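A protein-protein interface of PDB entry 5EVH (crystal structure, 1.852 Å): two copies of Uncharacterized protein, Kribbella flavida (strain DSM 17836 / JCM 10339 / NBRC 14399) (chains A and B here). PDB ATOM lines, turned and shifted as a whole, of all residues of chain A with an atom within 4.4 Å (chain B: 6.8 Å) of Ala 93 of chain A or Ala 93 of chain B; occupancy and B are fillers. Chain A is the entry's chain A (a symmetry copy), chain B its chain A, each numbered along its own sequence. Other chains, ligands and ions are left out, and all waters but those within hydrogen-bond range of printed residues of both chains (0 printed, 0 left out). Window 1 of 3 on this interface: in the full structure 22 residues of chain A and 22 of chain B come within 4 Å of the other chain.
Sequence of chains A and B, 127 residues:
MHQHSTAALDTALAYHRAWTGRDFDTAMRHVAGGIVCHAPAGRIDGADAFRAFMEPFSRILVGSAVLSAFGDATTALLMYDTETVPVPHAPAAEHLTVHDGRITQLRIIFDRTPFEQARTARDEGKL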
ATOM      1  N   LEU A  78     -19.439 -24.209   6.994  1.00  0.00           N
ATOM      2  CA  LEU A  78     -20.598 -23.441   6.554  1.00  0.00           C
ATOM      3  C   LEU A  78     -20.536 -22.013   7.055  1.00  0.00           C
ATOM      4  O   LEU A  78     -19.825 -21.688   8.022  1.00  0.00           O
ATOM      5  CB  LEU A  78     -21.892 -24.039   7.003  1.00  0.00           C
ATOM      6  CG  LEU A  78     -22.011 -24.569   8.377  1.00  0.00           C
ATOM      7  CD1 LEU A  78     -22.904 -23.583   9.003  1.00  0.00           C
ATOM      8  CD2 LEU A  78     -22.788 -25.812   8.188  1.00  0.00           C
ATOM      9  N   MET A  79     -21.240 -21.160   6.316  1.00  0.00           N
ATOM     10  CA  MET A  79     -21.299 -19.734   6.690  1.00  0.00           C
ATOM     11  C   MET A  79     -22.775 -19.346   6.584  1.00  0.00           C
ATOM     12  O   MET A  79     -23.464 -19.733   5.605  1.00  0.00           O
ATOM     13  CB  MET A  79     -20.453 -18.906   5.762  1.00  0.00           C
ATOM     14  CG  MET A  79     -20.588 -17.393   6.159  1.00  0.00           C
ATOM     15  SD  MET A  79     -19.535 -16.202   4.991  1.00  0.00           S
ATOM     16  CE  MET A  79     -17.680 -16.738   5.575  1.00  0.00           C
ATOM     17  N   ALA A  92     -21.887 -15.767  10.816  1.00  0.00           N
ATOM     18  CA  ALA A  92     -20.954 -16.650  11.502  1.00  0.00           C
ATOM     19  C   ALA A  92     -20.452 -17.716  10.529  1.00  0.00           C
ATOM     20  O   ALA A  92     -21.135 -18.058   9.558  1.00  0.00           O
ATOM     21  CB  ALA A  92     -21.574 -17.334  12.742  1.00  0.00           C
ATOM     22  N   ALA A  93     -19.266 -18.251  10.787  1.00  0.00           N
ATOM     23  CA  ALA A  93     -18.806 -19.402  10.008  1.00  0.00           C
ATOM     24  C   ALA A  93     -18.417 -20.517  10.974  1.00  0.00           C
ATOM     25  O   ALA A  93     -17.900 -20.234  12.076  1.00  0.00           O
ATOM     26  CB  ALA A  93     -17.563 -19.023   9.145  1.00  0.00           C
ATOM     27  N   GLU A  94     -18.666 -21.785  10.574  1.00  0.00           N
ATOM     28  CA  GLU A  94     -18.401 -22.913  11.440  1.00  0.00           C
ATOM     29  C   GLU A  94     -17.655 -23.969  10.671  1.00  0.00           C
ATOM     30  O   GLU A  94     -18.037 -24.310   9.530  1.00  0.00           O
ATOM     31  CB  GLU A  94     -19.706 -23.598  12.029  1.00  0.00           C
ATOM     32  CG  GLU A  94     -20.459 -22.653  12.914  1.00  0.00           C
ATOM     33  CD  GLU A  94     -21.797 -23.258  13.390  1.00  0.00           C
ATOM     34  OE1 GLU A  94     -22.061 -24.381  12.953  1.00  0.00           O
ATOM     35  OE2 GLU A  94     -22.546 -22.616  14.187  1.00  0.00           O
ATOM     36  N   ARG A 107     -15.395 -25.258  15.365  1.00  0.00           N
ATOM     37  CA  ARG A 107     -14.763 -23.946  15.504  1.00  0.00           C
ATOM     38  C   ARG A 107     -15.713 -22.921  14.896  1.00  0.00           C
ATOM     39  O   ARG A 107     -16.075 -23.030  13.714  1.00  0.00           O
ATOM     40  CB  ARG A 107     -13.376 -23.877  14.853  1.00  0.00           C
ATOM     41  CG  ARG A 107     -12.805 -22.434  14.946  1.00  0.00           C
ATOM     42  CD  ARG A 107     -11.278 -22.320  14.497  1.00  0.00           C
ATOM     43  NE  ARG A 107     -10.378 -23.460  14.839  1.00  0.00           N
ATOM     44  CZ  ARG A 107      -9.597 -23.504  15.922  1.00  0.00           C
ATOM     45  NH1 ARG A 107      -8.813 -24.553  16.118  1.00  0.00           N
ATOM     46  NH2 ARG A 107      -9.589 -22.505  16.822  1.00  0.00           N
ATOM     47  N   ILE A 108     -16.098 -21.918  15.680  1.00  0.00           N
ATOM     48  CA  ILE A 108     -17.053 -20.926  15.172  1.00  0.00           C
ATOM     49  C   ILE A 108     -16.444 -19.532  15.224  1.00  0.00           C
ATOM     50  O   ILE A 108     -15.730 -19.190  16.170  1.00  0.00           O
ATOM     51  CB  ILE A 108     -18.403 -20.985  15.913  1.00  0.00           C
ATOM     52  CG1 ILE A 108     -19.310 -19.812  15.474  1.00  0.00           C
ATOM     53  CG2 ILE A 108     -18.252 -20.916  17.451  1.00  0.00           C
ATOM     54  CD1 ILE A 108     -20.769 -20.051  15.918  1.00  0.00           C
ATOM     55  N   ILE A 109     -16.642 -18.752  14.148  1.00  0.00           N
ATOM     56  CA  ILE A 109     -16.067 -17.396  14.051  1.00  0.00           C
ATOM     57  C   ILE A 109     -17.221 -16.430  13.844  1.00  0.00           C
ATOM     58  O   ILE A 109     -18.019 -16.619  12.928  1.00  0.00           O
ATOM     59  CB  ILE A 109     -15.079 -17.276  12.870  1.00  0.00           C
ATOM     60  CG1 ILE A 109     -13.993 -18.343  13.002  1.00  0.00           C
ATOM     61  CG2 ILE A 109     -14.495 -15.849  12.905  1.00  0.00           C
ATOM     62  CD1 ILE A 109     -12.957 -18.309  11.789  1.00  0.00           C
ATOM     63  N   LEU B  77     -15.253 -21.641  -0.116  1.00  0.00           N
ATOM     64  CA  LEU B  77     -15.421 -21.310   1.282  1.00  0.00           C
ATOM     65  C   LEU B  77     -14.156 -21.779   1.996  1.00  0.00           C
ATOM     66  O   LEU B  77     -13.746 -22.947   1.863  1.00  0.00           O
ATOM     67  CB  LEU B  77     -16.695 -22.019   1.822  1.00  0.00           C
ATOM     68  CG  LEU B  77     -17.148 -21.619   3.218  1.00  0.00           C
ATOM     69  CD1 LEU B  77     -17.529 -20.093   3.263  1.00  0.00           C
ATOM     70  CD2 LEU B  77     -18.389 -22.490   3.637  1.00  0.00           C
ATOM     71  N   LEU B  78     -13.519 -20.888   2.738  1.00  0.00           N
ATOM     72  CA  LEU B  78     -12.336 -21.347   3.455  1.00  0.00           C
ATOM     73  C   LEU B  78     -12.227 -20.692   4.816  1.00  0.00           C
ATOM     74  O   LEU B  78     -12.825 -19.635   5.085  1.00  0.00           O
ATOM     75  CB  LEU B  78     -11.070 -21.084   2.707  1.00  0.00           C
ATOM     76  CG  LEU B  78     -10.888 -19.792   2.014  1.00  0.00           C
ATOM     77  CD1 LEU B  78      -9.862 -19.147   2.846  1.00  0.00           C
ATOM     78  CD2 LEU B  78     -10.245 -20.183   0.742  1.00  0.00           C
ATOM     79  N   MET B  79     -11.511 -21.396   5.688  1.00  0.00           N
ATOM     80  CA  MET B  79     -11.293 -20.878   7.052  1.00  0.00           C
ATOM     81  C   MET B  79      -9.801 -21.075   7.329  1.00  0.00           C
ATOM     82  O   MET B  79      -9.232 -22.149   7.002  1.00  0.00           O
ATOM     83  CB  MET B  79     -12.133 -21.631   8.048  1.00  0.00           C
ATOM     84  CG  MET B  79     -11.829 -21.089   9.489  1.00  0.00           C
ATOM     85  SD  MET B  79     -12.861 -22.021  10.888  1.00  0.00           S
ATOM     86  CE  MET B  79     -14.703 -21.332  10.440  1.00  0.00           C
ATOM     87  N   TYR B  80      -9.143 -20.048   7.903  1.00  0.00           N
ATOM     88  CA  TYR B  80      -7.711 -20.095   8.136  1.00  0.00           C
ATOM     89  C   TYR B  80      -7.415 -19.427   9.468  1.00  0.00           C
ATOM     90  O   TYR B  80      -8.138 -18.544   9.929  1.00  0.00           O
ATOM     91  CB  TYR B  80      -6.895 -19.456   6.979  1.00  0.00           C
ATOM     92  CG  TYR B  80      -7.325 -18.066   6.603  1.00  0.00           C
ATOM     93  CD1 TYR B  80      -8.271 -17.858   5.605  1.00  0.00           C
ATOM     94  CD2 TYR B  80      -6.771 -16.967   7.241  1.00  0.00           C
ATOM     95  CE1 TYR B  80      -8.643 -16.557   5.243  1.00  0.00           C
ATOM     96  CE2 TYR B  80      -7.128 -15.666   6.897  1.00  0.00           C
ATOM     97  CZ  TYR B  80      -8.079 -15.479   5.904  1.00  0.00           C
ATOM     98  OH  TYR B  80      -8.462 -14.191   5.560  1.00  0.00           O
ATOM     99  N   PRO B  91      -8.435 -16.107  13.735  1.00  0.00           N
ATOM    100  CA  PRO B  91      -8.909 -16.889  12.578  1.00  0.00           C
ATOM    101  C   PRO B  91      -9.944 -16.118  11.759  1.00  0.00           C
ATOM    102  O   PRO B  91     -10.650 -15.249  12.275  1.00  0.00           O
ATOM    103  CB  PRO B  91      -9.527 -18.126  13.224  1.00  0.00           C
ATOM    104  CG  PRO B  91     -10.138 -17.554  14.486  1.00  0.00           C
ATOM    105  CD  PRO B  91      -8.966 -16.619  15.014  1.00  0.00           C
ATOM    106  N   ALA B  92     -10.015 -16.421  10.459  1.00  0.00           N
ATOM    107  CA  ALA B  92     -10.965 -15.752   9.581  1.00  0.00           C
ATOM    108  C   ALA B  92     -11.638 -16.784   8.679  1.00  0.00           C
ATOM    109  O   ALA B  92     -11.071 -17.843   8.396  1.00  0.00           O
ATOM    110  CB  ALA B  92     -10.311 -14.653   8.711  1.00  0.00           C
ATOM    111  N   ALA B  93     -12.843 -16.479   8.215  1.00  0.00           N
ATOM    112  CA  ALA B  93     -13.468 -17.331   7.202  1.00  0.00           C
ATOM    113  C   ALA B  93     -13.877 -16.460   6.019  1.00  0.00           C
ATOM    114  O   ALA B  93     -14.275 -15.291   6.215  1.00  0.00           O
ATOM    115  CB  ALA B  93     -14.738 -18.032   7.778  1.00  0.00           C
ATOM    116  N   GLU B  94     -13.778 -17.014   4.790  1.00  0.00           N
ATOM    117  CA  GLU B  94     -14.072 -16.253   3.595  1.00  0.00           C
ATOM    118  C   GLU B  94     -14.971 -17.061   2.698  1.00  0.00           C
ATOM    119  O   GLU B  94     -14.715 -18.262   2.461  1.00  0.00           O
ATOM    120  CB  GLU B  94     -12.792 -15.862   2.743  1.00  0.00           C
ATOM    121  CG  GLU B  94     -11.886 -14.953   3.516  1.00  0.00           C
ATOM    122  CD  GLU B  94     -10.575 -14.668   2.754  1.00  0.00           C
ATOM    123  OE1 GLU B  94     -10.450 -15.245   1.671  1.00  0.00           O
ATOM    124  OE2 GLU B  94      -9.708 -13.878   3.237  1.00  0.00           O
ATOM    125  N   HIS B  95     -15.979 -16.376   2.132  1.00  0.00           N
ATOM    126  CA  HIS B  95     -16.848 -16.969   1.142  1.00  0.00           C
ATOM    127  C   HIS B  95     -16.579 -16.200  -0.147  1.00  0.00           C
ATOM    128  O   HIS B  95     -16.769 -14.974  -0.175  1.00  0.00           O
ATOM    129  CB  HIS B  95     -18.312 -16.842   1.556  1.00  0.00           C
ATOM    130  CG  HIS B  95     -19.271 -17.312   0.492  1.00  0.00           C
ATOM    131  ND1 HIS B  95     -20.485 -16.693   0.257  1.00  0.00           N
ATOM    132  CD2 HIS B  95     -19.223 -18.376  -0.366  1.00  0.00           C
ATOM    133  CE1 HIS B  95     -21.134 -17.332  -0.714  1.00  0.00           C
ATOM    134  NE2 HIS B  95     -20.376 -18.342  -1.130  1.00  0.00           N
ATOM    135  N   LEU B 106     -16.600 -11.266  -2.113  1.00  0.00           N
ATOM    136  CA  LEU B 106     -15.798 -11.821  -1.030  1.00  0.00           C
ATOM    137  C   LEU B 106     -16.467 -11.387   0.257  1.00  0.00           C
ATOM    138  O   LEU B 106     -16.587 -10.177   0.489  1.00  0.00           O
ATOM    139  CB  LEU B 106     -14.356 -11.308  -1.096  1.00  0.00           C
ATOM    140  CG  LEU B 106     -13.394 -12.088  -0.164  1.00  0.00           C
ATOM    141  CD1 LEU B 106     -11.965 -11.895  -0.727  1.00  0.00           C
ATOM    142  CD2 LEU B 106     -13.397 -11.621   1.203  1.00  0.00           C
ATOM    143  N   ARG B 107     -16.951 -12.347   1.066  1.00  0.00           N
ATOM    144  CA  ARG B 107     -17.447 -12.011   2.400  1.00  0.00           C
ATOM    145  C   ARG B 107     -16.461 -12.589   3.409  1.00  0.00           C
ATOM    146  O   ARG B 107     -16.207 -13.804   3.407  1.00  0.00           O
ATOM    147  CB  ARG B 107     -18.871 -12.522   2.656  1.00  0.00           C
ATOM    148  CG  ARG B 107     -19.299 -12.223   4.120  1.00  0.00           C
ATOM    149  CD  ARG B 107     -20.841 -12.517   4.409  1.00  0.00           C
ATOM    150  NE  ARG B 107     -21.809 -12.219   3.314  1.00  0.00           N
ATOM    151  CZ  ARG B 107     -22.501 -11.081   3.209  1.00  0.00           C
ATOM    152  NH1 ARG B 107     -23.358 -10.928   2.212  1.00  0.00           N
ATOM    153  NH2 ARG B 107     -22.345 -10.082   4.096  1.00  0.00           N
ATOM    154  N   ILE B 108     -15.924 -11.740   4.280  1.00  0.00           N
ATOM    155  CA  ILE B 108     -14.927 -12.224   5.243  1.00  0.00           C
ATOM    156  C   ILE B 108     -15.401 -11.967   6.667  1.00  0.00           C
ATOM    157  O   ILE B 108     -16.001 -10.929   6.955  1.00  0.00           O
ATOM    158  CB  ILE B 108     -13.533 -11.619   4.991  1.00  0.00           C
ATOM    159  CG1 ILE B 108     -12.562 -12.010   6.128  1.00  0.00           C
ATOM    160  CG2 ILE B 108     -13.551 -10.075   4.895  1.00  0.00           C
ATOM    161  CD1 ILE B 108     -11.099 -11.728   5.723  1.00  0.00           C
ATOM    162  N   ILE B 109     -15.221 -12.966   7.546  1.00  0.00           N
ATOM    163  CA  ILE B 109     -15.676 -12.865   8.947  1.00  0.00           C
ATOM    164  C   ILE B 109     -14.461 -13.071   9.833  1.00  0.00           C
ATOM    165  O   ILE B 109     -13.759 -14.070   9.686  1.00  0.00           O
ATOM    166  CB  ILE B 109     -16.742 -13.931   9.281  1.00  0.00           C
ATOM    167  CG1 ILE B 109     -17.906 -13.817   8.298  1.00  0.00           C
ATOM    168  CG2 ILE B 109     -17.190 -13.690  10.738  1.00  0.00           C
ATOM    169  CD1 ILE B 109     -19.030 -14.920   8.555  1.00  0.00           C
ATOM    170  N   PHE B 110     -14.232 -12.151  10.769  1.00  0.00           N
ATOM    171  CA  PHE B 110     -13.299 -12.392  11.853  1.00  0.00           C
ATOM    172  C   PHE B 110     -13.711 -11.503  13.020  1.00  0.00           C
ATOM    173  O   PHE B 110     -14.512 -10.560  12.871  1.00  0.00           O
ATOM    174  CB  PHE B 110     -11.851 -12.096  11.459  1.00  0.00           C
ATOM    175  CG  PHE B 110     -11.636 -10.708  10.939  1.00  0.00           C
ATOM    176  CD1 PHE B 110     -11.703 -10.462   9.563  1.00  0.00           C
ATOM    177  CD2 PHE B 110     -11.374  -9.663  11.809  1.00  0.00           C
ATOM    178  CE1 PHE B 110     -11.486  -9.126   9.064  1.00  0.00           C
ATOM    179  CE2 PHE B 110     -11.165  -8.335  11.346  1.00  0.00           C
ATOM    180  CZ  PHE B 110     -11.243  -8.068   9.980  1.00  0.00           C
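The backbone carbonyl oxygen (O) of Leu 78 of chain B lies within hydrogen-bond range of the backbone NH (N) of Glu 94 of chain B. The side-chain hydroxyl (OH) of Tyr 80 of chain B sits at hydrogen-bond distance from the side-chain carboxylate (OE2) of Glu 94 of chain B (2.7 Å). The backbone carbonyl oxygen (O) of Ala 93 of chain B is in hydrogen-bond range of the backbone NH (N) of Ile 109 of chain B (2.8 Å). The backbone NH of His 95 of chain B is in hydrogen-bond range of the backbone carbonyl oxygen of Arg 107 of chain B, 2.9 Å away. The backbone NH of Glu 94 of chain A is in hydrogen-bond range of the backbone carbonyl oxygen of Leu 78 of chain A. The backbone carbonyl oxygen of Ala 93 of chain A sits at hydrogen-bond distance from the backbone NH of Ile 109 of chain A (2.8 Å).
Printed residues of chain B within 4 Å of Met 79 of chain A: Ala 93, Glu 94, His 95, Arg 107 and Ile 109. Printed residues of chain B within 4 Å of Ala 93 of chain A: Met 79 (3.8 Å) and Ala 93 (3.3 Å). Ile 108 of chain A touches none of the printed residues of chain B. Printed residues of chain B within 4 Å of Ile 109 of chain A: Met 79 (3.7 Å), Pro 91 (3.7 Å), Ala 92 (3.7 Å), Ile 109 (3.7 Å) and Phe 110 (3.8 Å). Printed residues of chain A within 4 Å of Ala 92 of chain B: Ile 109. Of the printed residues of chain A, Ala 93 of chain B touches Met 79 (3.8 Å) and Ala 93 (3.3 Å). Printed residues of chain A within 4 Å of Glu 94 of chain B: Met 79. Of the printed residues of chain A, Phe 110 of chain B touches Ile 109 (3.8 Å).
Leu 77 of chain B touches Leu 78 of chain A (CD2 to CA, 3.8 Å). CE of Met 79 of chain A touches O of Ala 93 of chain B (3.8 Å). Met 79 of chain A touches His 95 of chain B. Arg 107 of chain B touches Met 79 of chain A (O to CE, 3.9 Å). Met 79 of chain A touches Ile 109 of chain B (CE to CD1, 3.7 Å). Ala 92 of chain A touches Ile 109 of chain B. Ala 93 of chain A touches Ala 93 of chain B (CB to CB, 3.3 Å). Glu 94 of chain A touches Met 79 of chain B. O of Ile 109 of chain A touches CG2 of Ile 109 of chain B, 3.7 Å away. Phe 110 of chain B touches Ile 109 of chain A.
Met 79 of chain A touches Ile 109 of chain B, and with the chains exchanged Ile 109 of chain A touches Met 79 of chain B. Ala 92 of chain A touches Ile 109 of chain B, and with the chains exchanged Ile 109 of chain A touches Ala 92 of chain B. Ala 93 of chain A touches its own counterpart, Ala 93 of chain B. Ile 109 of chain B touches its own counterpart, Ile 109 of chain A. 8 positions are printed for both chains.
Of the 8 printed residues of chain A, 7 touch a printed residue of chain B. Printed residues of chain A that touch a printed residue of chain B: Leu 78, Met 79, Ala 92, Ala 93, Glu 94, Arg 107 and Ile 109. Hydrophobic or aromatic side chains of chain A that line the printed part of chain B: Met 79, Ala 93 and Ile 109. Of the 14 printed residues of chain B, 10 touch a printed residue of chain A. Printed residues of chain B that touch a printed residue of chain A: Leu 77, Met 79, Pro 91, Ala 92, Ala 93, Glu 94, His 95, Arg 107, Ile 109 and Phe 110. Along chain B the printed residues that touch a printed residue of chain A span positions 77 to 110. Among the printed residues, 16 pairs touch across the chains.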
